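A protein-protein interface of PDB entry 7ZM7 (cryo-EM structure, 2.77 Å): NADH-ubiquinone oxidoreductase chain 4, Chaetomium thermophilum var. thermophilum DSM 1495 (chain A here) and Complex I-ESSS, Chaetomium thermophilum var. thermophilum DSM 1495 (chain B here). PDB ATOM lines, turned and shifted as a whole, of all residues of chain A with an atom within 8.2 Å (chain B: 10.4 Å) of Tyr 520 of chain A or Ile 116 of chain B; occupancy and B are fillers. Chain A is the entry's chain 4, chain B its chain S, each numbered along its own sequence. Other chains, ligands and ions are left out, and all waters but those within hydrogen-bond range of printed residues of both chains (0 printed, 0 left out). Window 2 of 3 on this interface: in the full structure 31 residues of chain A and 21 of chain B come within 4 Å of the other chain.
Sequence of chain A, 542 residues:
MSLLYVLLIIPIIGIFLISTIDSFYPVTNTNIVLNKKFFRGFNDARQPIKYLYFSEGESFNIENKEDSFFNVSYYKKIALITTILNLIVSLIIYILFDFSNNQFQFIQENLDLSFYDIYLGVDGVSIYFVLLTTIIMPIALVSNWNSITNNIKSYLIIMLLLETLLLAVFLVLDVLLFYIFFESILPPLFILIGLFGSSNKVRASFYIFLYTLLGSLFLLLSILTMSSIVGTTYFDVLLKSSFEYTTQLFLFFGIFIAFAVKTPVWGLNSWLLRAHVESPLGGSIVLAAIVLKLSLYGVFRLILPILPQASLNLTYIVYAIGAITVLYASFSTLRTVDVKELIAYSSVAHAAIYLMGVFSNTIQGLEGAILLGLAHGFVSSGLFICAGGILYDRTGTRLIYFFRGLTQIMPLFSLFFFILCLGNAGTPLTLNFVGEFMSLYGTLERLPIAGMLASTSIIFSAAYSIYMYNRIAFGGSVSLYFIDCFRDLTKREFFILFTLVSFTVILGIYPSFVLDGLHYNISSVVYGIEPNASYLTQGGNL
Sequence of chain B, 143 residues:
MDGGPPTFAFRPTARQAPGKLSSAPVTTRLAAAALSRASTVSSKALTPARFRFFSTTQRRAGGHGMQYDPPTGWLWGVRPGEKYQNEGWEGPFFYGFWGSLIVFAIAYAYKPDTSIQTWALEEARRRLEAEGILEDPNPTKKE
The side-chain hydroxyl (OG1) of Thr 114 of chain B sits at hydrogen-bond distance from the backbone NH (N) of Phe 99 of chain A, at 2.5 Å.
The backbone carbonyl oxygen (O) of Thr 114 of chain B lies within hydrogen-bond range of the side-chain hydroxyl (OG) of Ser 100 of chain A, 2.8 Å away.
NE2 of His 519 of chain A lies close to NE2 of Gln 117 of chain B (3.3 Å).
OE1 of Gln 117 of chain B is in hydrogen-bond range of OG of Ser 115 of chain B (2.8 Å).
N of Ser 100 of chain A sits close to OD1 of Asp 98 of chain A (3.4 Å).
N of Asn 101 of chain A sits close to OD1 of Asp 98 of chain A (3.4 Å).
OE2 of Glu 367 of chain A sits at hydrogen-bond distance from ND1 of His 519 of chain A (2.8 Å).
The backbone carbonyl oxygen (O) of Leu 515 of chain A sits close to a ring nitrogen (NE2) of His 519 of chain A, 3.2 Å away.
O of His 519 of chain A sits at hydrogen-bond distance from OG of Ser 523 of chain A, at 2.6 Å.
Among the printed residues, merely in contact across the chains: Asp 98 of chain A with Thr 114 of chain B (3.5 Å), Phe 99 of chain A with Ser 115 of chain B (3.95 Å), Ser 100 of chain A with Ile 116 of chain B (3.99 Å), Asp 516 of chain A with Ser 115 of chain B (3.9 Å), His 519 of chain A with Ile 116 of chain B (3.8 Å) and Tyr 520 of chain A with Ile 116 of chain B (3.7 Å).
Of the printed residues of chain B, Phe 99 of chain A touches Thr 114 and Ser 115.
Asn 101 of chain A touches none of the printed residues of chain B.
No residue of chain B comes within 4 Å of Asn 102 of chain A.
Printed residues of chain B within 4 Å of Asp 516 of chain A: Ser 115.
No residue of chain B comes within 4 Å of Gly 517 of chain A.
Of the printed residues of chain B, His 519 of chain A touches Ile 116 (3.8 Å) and Gln 117 (3.1 Å).
Tyr 520 of chain A touches just one residue of chain B: Ile 116.
No residue of chain B comes within 4 Å of Ser 523 of chain A.
Printed residues of chain A within 4 Å of Thr 114 of chain B: Asp 98 (3.5 Å), Phe 99 (2.5 Å) and Ser 100 (2.8 Å).
Of chain A, only Phe 99 and Asp 516 come within 4 Å of Ser 115 of chain B.
Of the printed residues of chain A, Ile 116 of chain B touches Ser 100, His 519 and Tyr 520.
The nearest residue of chain B that does not touch Tyr 520 of chain A is Thr 114 of chain B (6.3 Å).
The nearest printed residue of chain B that does not touch Ser 100 of chain A is Ser 115 of chain B (4.3 Å).
Of the 13 printed residues of chain B, 4 touch a printed residue of chain A.
Hydrophobic or aromatic side chains of chain B within 4 Å of the printed part of chain A: Ile 116.
Of the 23 printed residues of chain A, 6 touch a printed residue of chain B.
Among the printed residues, no Asp or Glu carboxylate lies within 4 Å of a Lys or Arg side-chain nitrogen of the other chain.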
ATOM      1  N   ASP A  98       3.443  -2.610  20.147  1.00  0.00           N
ATOM      2  CA  ASP A  98       4.372  -3.723  19.980  1.00  0.00           C
ATOM      3  C   ASP A  98       5.395  -3.654  21.102  1.00  0.00           C
ATOM      4  O   ASP A  98       6.243  -2.761  21.118  1.00  0.00           O
ATOM      5  CB  ASP A  98       5.053  -3.670  18.618  1.00  0.00           C
ATOM      6  CG  ASP A  98       5.825  -4.923  18.302  1.00  0.00           C
ATOM      7  OD1 ASP A  98       6.925  -5.110  18.844  1.00  0.00           O
ATOM      8  OD2 ASP A  98       5.334  -5.724  17.492  1.00  0.00           O
ATOM      9  N   PHE A  99       5.333  -4.605  22.021  1.00  0.00           N
ATOM     10  CA  PHE A  99       6.060  -4.505  23.277  1.00  0.00           C
ATOM     11  C   PHE A  99       7.563  -4.667  23.140  1.00  0.00           C
ATOM     12  O   PHE A  99       8.271  -4.406  24.113  1.00  0.00           O
ATOM     13  CB  PHE A  99       5.559  -5.546  24.276  1.00  0.00           C
ATOM     14  CG  PHE A  99       4.272  -5.198  24.937  1.00  0.00           C
ATOM     15  CD1 PHE A  99       3.768  -3.919  24.868  1.00  0.00           C
ATOM     16  CD2 PHE A  99       3.584  -6.142  25.660  1.00  0.00           C
ATOM     17  CE1 PHE A  99       2.600  -3.590  25.488  1.00  0.00           C
ATOM     18  CE2 PHE A  99       2.415  -5.819  26.282  1.00  0.00           C
ATOM     19  CZ  PHE A  99       1.920  -4.535  26.194  1.00  0.00           C
ATOM     20  N   SER A 100       8.081  -5.115  21.997  1.00  0.00           N
ATOM     21  CA  SER A 100       9.522  -5.301  21.832  1.00  0.00           C
ATOM     22  C   SER A 100       9.975  -4.833  20.449  1.00  0.00           C
ATOM     23  O   SER A 100      10.603  -5.565  19.694  1.00  0.00           O
ATOM     24  CB  SER A 100       9.934  -6.746  22.088  1.00  0.00           C
ATOM     25  OG  SER A 100       9.297  -7.637  21.205  1.00  0.00           O
ATOM     26  N   ASN A 101       9.658  -3.590  20.121  1.00  0.00           N
ATOM     27  CA  ASN A 101      10.036  -2.962  18.864  1.00  0.00           C
ATOM     28  C   ASN A 101      10.914  -1.761  19.177  1.00  0.00           C
ATOM     29  O   ASN A 101      10.544  -0.936  20.006  1.00  0.00           O
ATOM     30  CB  ASN A 101       8.778  -2.540  18.101  1.00  0.00           C
ATOM     31  CG  ASN A 101       9.012  -2.338  16.622  1.00  0.00           C
ATOM     32  OD1 ASN A 101      10.134  -2.332  16.145  1.00  0.00           O
ATOM     33  ND2 ASN A 101       7.934  -2.183  15.887  1.00  0.00           N
ATOM     34  N   ASN A 102      12.064  -1.640  18.524  1.00  0.00           N
ATOM     35  CA  ASN A 102      13.022  -0.552  18.870  1.00  0.00           C
ATOM     36  C   ASN A 102      12.847   0.622  17.918  1.00  0.00           C
ATOM     37  O   ASN A 102      13.707   1.501  17.919  1.00  0.00           O
ATOM     38  CB  ASN A 102      14.478  -1.017  18.961  1.00  0.00           C
ATOM     39  CG  ASN A 102      15.221  -1.029  17.643  1.00  0.00           C
ATOM     40  OD1 ASN A 102      14.660  -1.353  16.601  1.00  0.00           O
ATOM     41  ND2 ASN A 102      16.499  -0.700  17.686  1.00  0.00           N
ATOM     42  N   GLN A 103      11.764   0.634  17.157  1.00  0.00           N
ATOM     43  CA  GLN A 103      11.469   1.783  16.274  1.00  0.00           C
ATOM     44  C   GLN A 103      10.269   2.509  16.871  1.00  0.00           C
ATOM     45  O   GLN A 103       9.509   1.856  17.600  1.00  0.00           O
ATOM     46  CB  GLN A 103      11.130   1.305  14.860  1.00  0.00           C
ATOM     47  CG  GLN A 103      12.301   0.705  14.102  1.00  0.00           C
ATOM     48  CD  GLN A 103      13.160   1.774  13.479  1.00  0.00           C
ATOM     49  OE1 GLN A 103      12.719   2.899  13.262  1.00  0.00           O
ATOM     50  NE2 GLN A 103      14.399   1.425  13.181  1.00  0.00           N
ATOM     51  N   GLN A 105       6.614   4.009  17.075  1.00  0.00           N
ATOM     52  CA  GLN A 105       5.397   3.405  16.488  1.00  0.00           C
ATOM     53  C   GLN A 105       4.314   4.469  16.327  1.00  0.00           C
ATOM     54  O   GLN A 105       4.411   5.494  17.004  1.00  0.00           O
ATOM     55  CB  GLN A 105       4.915   2.262  17.379  1.00  0.00           C
ATOM     56  CG  GLN A 105       5.934   1.157  17.586  1.00  0.00           C
ATOM     57  CD  GLN A 105       5.437   0.148  18.591  1.00  0.00           C
ATOM     58  OE1 GLN A 105       4.253  -0.165  18.643  1.00  0.00           O
ATOM     59  NE2 GLN A 105       6.345  -0.360  19.407  1.00  0.00           N
ATOM     60  N   ASP A 123       6.397   5.141  22.254  1.00  0.00           N
ATOM     61  CA  ASP A 123       7.390   4.143  22.581  1.00  0.00           C
ATOM     62  C   ASP A 123       7.008   3.491  23.898  1.00  0.00           C
ATOM     63  O   ASP A 123       6.247   4.045  24.689  1.00  0.00           O
ATOM     64  CB  ASP A 123       8.772   4.766  22.673  1.00  0.00           C
ATOM     65  CG  ASP A 123       9.847   3.747  22.738  1.00  0.00           C
ATOM     66  OD1 ASP A 123      10.131   3.156  21.679  1.00  0.00           O
ATOM     67  OD2 ASP A 123      10.401   3.525  23.833  1.00  0.00           O
ATOM     68  N   GLY A 124       7.531   2.293  24.120  1.00  0.00           N
ATOM     69  CA  GLY A 124       7.195   1.567  25.327  1.00  0.00           C
ATOM     70  C   GLY A 124       7.666   2.235  26.592  1.00  0.00           C
ATOM     71  O   GLY A 124       7.236   1.854  27.678  1.00  0.00           O
ATOM     72  N   VAL A 125       8.563   3.213  26.483  1.00  0.00           N
ATOM     73  CA  VAL A 125       8.940   3.977  27.662  1.00  0.00           C
ATOM     74  C   VAL A 125       8.010   5.155  27.876  1.00  0.00           C
ATOM     75  O   VAL A 125       7.988   5.715  28.972  1.00  0.00           O
ATOM     76  CB  VAL A 125      10.408   4.440  27.581  1.00  0.00           C
ATOM     77  CG1 VAL A 125      10.576   5.574  26.595  1.00  0.00           C
ATOM     78  CG2 VAL A 125      10.948   4.817  28.957  1.00  0.00           C
ATOM     79  N   ILE A 363      18.624  -1.963  35.156  1.00  0.00           N
ATOM     80  CA  ILE A 363      17.303  -2.204  34.514  1.00  0.00           C
ATOM     81  C   ILE A 363      16.225  -2.228  35.598  1.00  0.00           C
ATOM     82  O   ILE A 363      15.074  -1.901  35.270  1.00  0.00           O
ATOM     83  CB  ILE A 363      17.343  -3.529  33.729  1.00  0.00           C
ATOM     84  CG1 ILE A 363      16.568  -3.449  32.413  1.00  0.00           C
ATOM     85  CG2 ILE A 363      16.869  -4.687  34.585  1.00  0.00           C
ATOM     86  CD1 ILE A 363      17.311  -2.726  31.326  1.00  0.00           C
ATOM     87  N   GLU A 367      12.922   0.567  35.802  1.00  0.00           N
ATOM     88  CA  GLU A 367      11.503   0.146  35.704  1.00  0.00           C
ATOM     89  C   GLU A 367      10.775   0.474  37.008  1.00  0.00           C
ATOM     90  O   GLU A 367       9.621   0.923  36.927  1.00  0.00           O
ATOM     91  CB  GLU A 367      11.400  -1.315  35.286  1.00  0.00           C
ATOM     92  CG  GLU A 367      12.078  -1.581  33.965  1.00  0.00           C
ATOM     93  CD  GLU A 367      12.088  -3.047  33.585  1.00  0.00           C
ATOM     94  OE1 GLU A 367      12.544  -3.871  34.400  1.00  0.00           O
ATOM     95  OE2 GLU A 367      11.620  -3.353  32.483  1.00  0.00           O
ATOM     96  N   LEU A 515       4.996  -3.952  33.166  1.00  0.00           N
ATOM     97  CA  LEU A 515       6.440  -4.298  33.055  1.00  0.00           C
ATOM     98  C   LEU A 515       6.788  -4.854  31.666  1.00  0.00           C
ATOM     99  O   LEU A 515       7.915  -4.602  31.217  1.00  0.00           O
ATOM    100  CB  LEU A 515       6.806  -5.287  34.164  1.00  0.00           C
ATOM    101  CG  LEU A 515       7.130  -4.663  35.517  1.00  0.00           C
ATOM    102  CD1 LEU A 515       7.483  -5.733  36.534  1.00  0.00           C
ATOM    103  CD2 LEU A 515       8.262  -3.662  35.381  1.00  0.00           C
ATOM    104  N   ASP A 516       5.855  -5.550  31.008  1.00  0.00           N
ATOM    105  CA  ASP A 516       6.136  -6.205  29.700  1.00  0.00           C
ATOM    106  C   ASP A 516       6.473  -5.161  28.631  1.00  0.00           C
ATOM    107  O   ASP A 516       7.383  -5.425  27.830  1.00  0.00           O
ATOM    108  CB  ASP A 516       5.007  -7.160  29.313  1.00  0.00           C
ATOM    109  CG  ASP A 516       4.922  -8.363  30.236  1.00  0.00           C
ATOM    110  OD1 ASP A 516       5.835  -8.512  31.070  1.00  0.00           O
ATOM    111  OD2 ASP A 516       3.949  -9.133  30.116  1.00  0.00           O
ATOM    112  N   GLY A 517       5.757  -4.038  28.595  1.00  0.00           N
ATOM    113  CA  GLY A 517       6.092  -2.956  27.653  1.00  0.00           C
ATOM    114  C   GLY A 517       7.425  -2.314  27.968  1.00  0.00           C
ATOM    115  O   GLY A 517       8.136  -1.960  27.024  1.00  0.00           O
ATOM    116  N   LEU A 518       7.719  -2.106  29.248  1.00  0.00           N
ATOM    117  CA  LEU A 518       8.964  -1.411  29.670  1.00  0.00           C
ATOM    118  C   LEU A 518      10.253  -2.179  29.371  1.00  0.00           C
ATOM    119  O   LEU A 518      11.220  -1.528  28.978  1.00  0.00           O
ATOM    120  CB  LEU A 518       8.890  -1.141  31.175  1.00  0.00           C
ATOM    121  CG  LEU A 518       7.786  -0.204  31.653  1.00  0.00           C
ATOM    122  CD1 LEU A 518       7.861  -0.046  33.162  1.00  0.00           C
ATOM    123  CD2 LEU A 518       7.885   1.146  30.968  1.00  0.00           C
ATOM    124  N   HIS A 519      10.266  -3.506  29.489  1.00  0.00           N
ATOM    125  CA  HIS A 519      11.559  -4.241  29.457  1.00  0.00           C
ATOM    126  C   HIS A 519      12.415  -3.963  28.225  1.00  0.00           C
ATOM    127  O   HIS A 519      13.587  -3.632  28.428  1.00  0.00           O
ATOM    128  CB  HIS A 519      11.302  -5.753  29.483  1.00  0.00           C
ATOM    129  CG  HIS A 519      10.651  -6.262  30.720  1.00  0.00           C
ATOM    130  ND1 HIS A 519      11.185  -6.053  31.970  1.00  0.00           N
ATOM    131  CD2 HIS A 519       9.541  -7.007  30.898  1.00  0.00           C
ATOM    132  CE1 HIS A 519      10.412  -6.611  32.874  1.00  0.00           C
ATOM    133  NE2 HIS A 519       9.400  -7.209  32.242  1.00  0.00           N
ATOM    134  N   TYR A 520      11.872  -4.081  27.015  1.00  0.00           N
ATOM    135  CA  TYR A 520      12.725  -3.917  25.812  1.00  0.00           C
ATOM    136  C   TYR A 520      13.185  -2.466  25.623  1.00  0.00           C
ATOM    137  O   TYR A 520      14.369  -2.249  25.340  1.00  0.00           O
ATOM    138  CB  TYR A 520      11.998  -4.457  24.580  1.00  0.00           C
ATOM    139  CG  TYR A 520      12.874  -4.463  23.363  1.00  0.00           C
ATOM    140  CD1 TYR A 520      13.790  -5.480  23.167  1.00  0.00           C
ATOM    141  CD2 TYR A 520      12.819  -3.432  22.443  1.00  0.00           C
ATOM    142  CE1 TYR A 520      14.618  -5.490  22.063  1.00  0.00           C
ATOM    143  CE2 TYR A 520      13.642  -3.427  21.335  1.00  0.00           C
ATOM    144  CZ  TYR A 520      14.548  -4.453  21.157  1.00  0.00           C
ATOM    145  OH  TYR A 520      15.382  -4.431  20.093  1.00  0.00           O
ATOM    146  N   ASN A 521      12.272  -1.508  25.746  1.00  0.00           N
ATOM    147  CA  ASN A 521      12.583  -0.067  25.528  1.00  0.00           C
ATOM    148  C   ASN A 521      13.485   0.489  26.632  1.00  0.00           C
ATOM    149  O   ASN A 521      14.354   1.315  26.321  1.00  0.00           O
ATOM    150  CB  ASN A 521      11.305   0.729  25.259  1.00  0.00           C
ATOM    151  CG  ASN A 521      10.701   0.371  23.918  1.00  0.00           C
ATOM    152  OD1 ASN A 521       9.525   0.034  23.832  1.00  0.00           O
ATOM    153  ND2 ASN A 521      11.500   0.419  22.865  1.00  0.00           N
ATOM    154  N   ILE A 522      13.258   0.079  27.877  1.00  0.00           N
ATOM    155  CA  ILE A 522      14.119   0.527  29.006  1.00  0.00           C
ATOM    156  C   ILE A 522      15.524  -0.020  28.747  1.00  0.00           C
ATOM    157  O   ILE A 522      16.495   0.611  29.180  1.00  0.00           O
ATOM    158  CB  ILE A 522      13.538   0.101  30.374  1.00  0.00           C
ATOM    159  CG1 ILE A 522      13.633   1.219  31.414  1.00  0.00           C
ATOM    160  CG2 ILE A 522      14.148  -1.199  30.877  1.00  0.00           C
ATOM    161  CD1 ILE A 522      12.615   2.311  31.228  1.00  0.00           C
ATOM    162  N   SER A 523      15.617  -1.176  28.097  1.00  0.00           N
ATOM    163  CA  SER A 523      16.930  -1.819  27.857  1.00  0.00           C
ATOM    164  C   SER A 523      17.803  -1.034  26.887  1.00  0.00           C
ATOM    165  O   SER A 523      18.905  -1.502  26.594  1.00  0.00           O
ATOM    166  CB  SER A 523      16.734  -3.220  27.331  1.00  0.00           C
ATOM    167  OG  SER A 523      16.168  -4.056  28.324  1.00  0.00           O
ATOM    168  N   SER A 524      17.356   0.151  26.463  1.00  0.00           N
ATOM    169  CA  SER A 524      18.222   0.987  25.650  1.00  0.00           C
ATOM    170  C   SER A 524      18.631   2.287  26.329  1.00  0.00           C
ATOM    171  O   SER A 524      19.197   3.152  25.661  1.00  0.00           O
ATOM    172  CB  SER A 524      17.549   1.275  24.311  1.00  0.00           C
ATOM    173  OG  SER A 524      16.289   1.877  24.479  1.00  0.00           O
ATOM    174  N   VAL A 525      18.378   2.461  27.622  1.00  0.00           N
ATOM    175  CA  VAL A 525      18.963   3.579  28.353  1.00  0.00           C
ATOM    176  C   VAL A 525      20.010   3.137  29.346  1.00  0.00           C
ATOM    177  O   VAL A 525      20.528   3.984  30.078  1.00  0.00           O
ATOM    178  CB  VAL A 525      17.904   4.451  29.064  1.00  0.00           C
ATOM    179  CG1 VAL A 525      17.072   5.208  28.067  1.00  0.00           C
ATOM    180  CG2 VAL A 525      17.020   3.616  29.971  1.00  0.00           C
ATOM    181  N   PRO B 112      -1.849 -10.326  20.950  1.00  0.00           N
ATOM    182  CA  PRO B 112      -0.659 -11.178  20.900  1.00  0.00           C
ATOM    183  C   PRO B 112       0.411 -10.679  21.850  1.00  0.00           C
ATOM    184  O   PRO B 112       0.477  -9.493  22.177  1.00  0.00           O
ATOM    185  CB  PRO B 112      -0.204 -11.066  19.446  1.00  0.00           C
ATOM    186  CG  PRO B 112      -0.833  -9.812  18.953  1.00  0.00           C
ATOM    187  CD  PRO B 112      -2.127  -9.696  19.655  1.00  0.00           C
ATOM    188  N   ASP B 113       1.251 -11.599  22.308  1.00  0.00           N
ATOM    189  CA  ASP B 113       2.291 -11.263  23.274  1.00  0.00           C
ATOM    190  C   ASP B 113       3.568 -10.912  22.532  1.00  0.00           C
ATOM    191  O   ASP B 113       4.216 -11.784  21.956  1.00  0.00           O
ATOM    192  CB  ASP B 113       2.541 -12.412  24.240  1.00  0.00           C
ATOM    193  CG  ASP B 113       3.505 -12.035  25.334  1.00  0.00           C
ATOM    194  OD1 ASP B 113       3.092 -11.292  26.253  1.00  0.00           O
ATOM    195  OD2 ASP B 113       4.675 -12.458  25.270  1.00  0.00           O
ATOM    196  N   THR B 114       3.931  -9.635  22.550  1.00  0.00           N
ATOM    197  CA  THR B 114       5.184  -9.165  21.975  1.00  0.00           C
ATOM    198  C   THR B 114       6.197  -8.806  23.048  1.00  0.00           C
ATOM    199  O   THR B 114       7.036  -7.931  22.839  1.00  0.00           O
ATOM    200  CB  THR B 114       4.945  -7.972  21.052  1.00  0.00           C
ATOM    201  OG1 THR B 114       4.347  -6.903  21.788  1.00  0.00           O
ATOM    202  CG2 THR B 114       4.011  -8.359  19.929  1.00  0.00           C
ATOM    203  N   SER B 115       6.122  -9.456  24.201  1.00  0.00           N
ATOM    204  CA  SER B 115       7.112  -9.257  25.242  1.00  0.00           C
ATOM    205  C   SER B 115       8.461  -9.837  24.822  1.00  0.00           C
ATOM    206  O   SER B 115       8.535 -10.816  24.085  1.00  0.00           O
ATOM    207  CB  SER B 115       6.645  -9.906  26.538  1.00  0.00           C
ATOM    208  OG  SER B 115       7.537  -9.593  27.590  1.00  0.00           O
ATOM    209  N   ILE B 116       9.545  -9.173  25.232  1.00  0.00           N
ATOM    210  CA  ILE B 116      10.923  -9.622  24.860  1.00  0.00           C
ATOM    211  C   ILE B 116      11.204 -10.964  25.530  1.00  0.00           C
ATOM    212  O   ILE B 116      12.052 -11.712  25.031  1.00  0.00           O
ATOM    213  CB  ILE B 116      11.989  -8.576  25.259  1.00  0.00           C
ATOM    214  CG1 ILE B 116      13.396  -8.956  24.795  1.00  0.00           C
ATOM    215  CG2 ILE B 116      11.950  -8.306  26.755  1.00  0.00           C
ATOM    216  CD1 ILE B 116      13.533  -9.136  23.307  1.00  0.00           C
ATOM    217  N   GLN B 117      10.457 -11.294  26.574  1.00  0.00           N
ATOM    218  CA  GLN B 117      10.811 -12.511  27.336  1.00  0.00           C
ATOM    219  C   GLN B 117      10.256 -13.727  26.605  1.00  0.00           C
ATOM    220  O   GLN B 117      11.024 -14.654  26.360  1.00  0.00           O
ATOM    221  CB  GLN B 117      10.249 -12.426  28.753  1.00  0.00           C
ATOM    222  CG  GLN B 117      11.142 -11.667  29.718  1.00  0.00           C
ATOM    223  CD  GLN B 117      10.647 -10.271  29.991  1.00  0.00           C
ATOM    224  OE1 GLN B 117       9.812  -9.738  29.264  1.00  0.00           O
ATOM    225  NE2 GLN B 117      11.166  -9.670  31.049  1.00  0.00           N
ATOM    226  N   THR B 118       8.998 -13.679  26.193  1.00  0.00           N
ATOM    227  CA  THR B 118       8.465 -14.808  25.444  1.00  0.00           C
ATOM    228  C   THR B 118       9.351 -15.152  24.269  1.00  0.00           C
ATOM    229  O   THR B 118       9.490 -16.327  23.920  1.00  0.00           O
ATOM    230  CB  THR B 118       7.050 -14.513  24.964  1.00  0.00           C
ATOM    231  OG1 THR B 118       6.280 -13.988  26.049  1.00  0.00           O
ATOM    232  CG2 THR B 118       6.391 -15.773  24.451  1.00  0.00           C
ATOM    233  N   TRP B 119       9.968 -14.146  23.655  1.00  0.00           N
ATOM    234  CA  TRP B 119      10.918 -14.396  22.581  1.00  0.00           C
ATOM    235  C   TRP B 119      12.242 -14.930  23.108  1.00  0.00           C
ATOM    236  O   TRP B 119      12.790 -15.889  22.560  1.00  0.00           O
ATOM    237  CB  TRP B 119      11.116 -13.125  21.765  1.00  0.00           C
ATOM    238  CG  TRP B 119      11.974 -13.368  20.570  1.00  0.00           C
ATOM    239  CD1 TRP B 119      11.558 -13.550  19.305  1.00  0.00           C
ATOM    240  CD2 TRP B 119      13.408 -13.387  20.533  1.00  0.00           C
ATOM    241  NE1 TRP B 119      12.629 -13.727  18.482  1.00  0.00           N
ATOM    242  CE2 TRP B 119      13.779 -13.630  19.216  1.00  0.00           C
ATOM    243  CE3 TRP B 119      14.407 -13.226  21.493  1.00  0.00           C
ATOM    244  CZ2 TRP B 119      15.104 -13.731  18.822  1.00  0.00           C
ATOM    245  CZ3 TRP B 119      15.713 -13.342  21.116  1.00  0.00           C
ATOM    246  CH2 TRP B 119      16.056 -13.589  19.788  1.00  0.00           C
ATOM    247  N   ALA B 120      12.774 -14.325  24.164  1.00  0.00           N
ATOM    248  CA  ALA B 120      14.078 -14.737  24.657  1.00  0.00           C
ATOM    249  C   ALA B 120      14.029 -16.108  25.308  1.00  0.00           C
ATOM    250  O   ALA B 120      15.044 -16.802  25.345  1.00  0.00           O
ATOM    251  CB  ALA B 120      14.626 -13.704  25.643  1.00  0.00           C
ATOM    252  N   LEU B 121      12.878 -16.498  25.858  1.00  0.00           N
ATOM    253  CA  LEU B 121      12.751 -17.834  26.424  1.00  0.00           C
ATOM    254  C   LEU B 121      12.822 -18.909  25.357  1.00  0.00           C
ATOM    255  O   LEU B 121      13.451 -19.949  25.562  1.00  0.00           O
ATOM    256  CB  LEU B 121      11.449 -17.979  27.205  1.00  0.00           C
ATOM    257  CG  LEU B 121      11.260 -17.540  28.659  1.00  0.00           C
ATOM    258  CD1 LEU B 121      12.147 -18.339  29.514  1.00  0.00           C
ATOM    259  CD2 LEU B 121      11.470 -16.100  28.924  1.00  0.00           C
ATOM    260  N   GLU B 122      12.161 -18.701  24.224  1.00  0.00           N
ATOM    261  CA  GLU B 122      12.111 -19.756  23.222  1.00  0.00           C
ATOM    262  C   GLU B 122      13.489 -20.051  22.656  1.00  0.00           C
ATOM    263  O   GLU B 122      13.842 -21.217  22.452  1.00  0.00           O
ATOM    264  CB  GLU B 122      11.148 -19.384  22.108  1.00  0.00           C
ATOM    265  CG  GLU B 122      11.103 -20.426  21.035  1.00  0.00           C
ATOM    266  CD  GLU B 122      10.365 -19.975  19.822  1.00  0.00           C
ATOM    267  OE1 GLU B 122       9.353 -19.266  19.989  1.00  0.00           O
ATOM    268  OE2 GLU B 122      10.802 -20.324  18.704  1.00  0.00           O
ATOM    269  N   GLU B 123      14.278 -19.010  22.393  1.00  0.00           N
ATOM    270  CA  GLU B 123      15.650 -19.218  21.955  1.00  0.00           C
ATOM    271  C   GLU B 123      16.499 -19.802  23.070  1.00  0.00           C
ATOM    272  O   GLU B 123      17.141 -20.845  22.892  1.00  0.00           O
ATOM    273  CB  GLU B 123      16.252 -17.902  21.464  1.00  0.00           C
ATOM    274  CG  GLU B 123      17.706 -18.005  21.039  1.00  0.00           C
ATOM    275  CD  GLU B 123      17.949 -19.046  19.938  1.00  0.00           C
ATOM    276  OE1 GLU B 123      17.303 -18.973  18.878  1.00  0.00           O
ATOM    277  OE2 GLU B 123      18.787 -19.945  20.145  1.00  0.00           O
ATOM    278  N   ALA B 124      16.510 -19.150  24.234  1.00  0.00           N
ATOM    279  CA  ALA B 124      17.327 -19.618  25.347  1.00  0.00           C
ATOM    280  C   ALA B 124      16.976 -21.038  25.730  1.00  0.00           C
ATOM    281  O   ALA B 124      17.830 -21.780  26.219  1.00  0.00           O
ATOM    282  CB  ALA B 124      17.151 -18.704  26.554  1.00  0.00           C
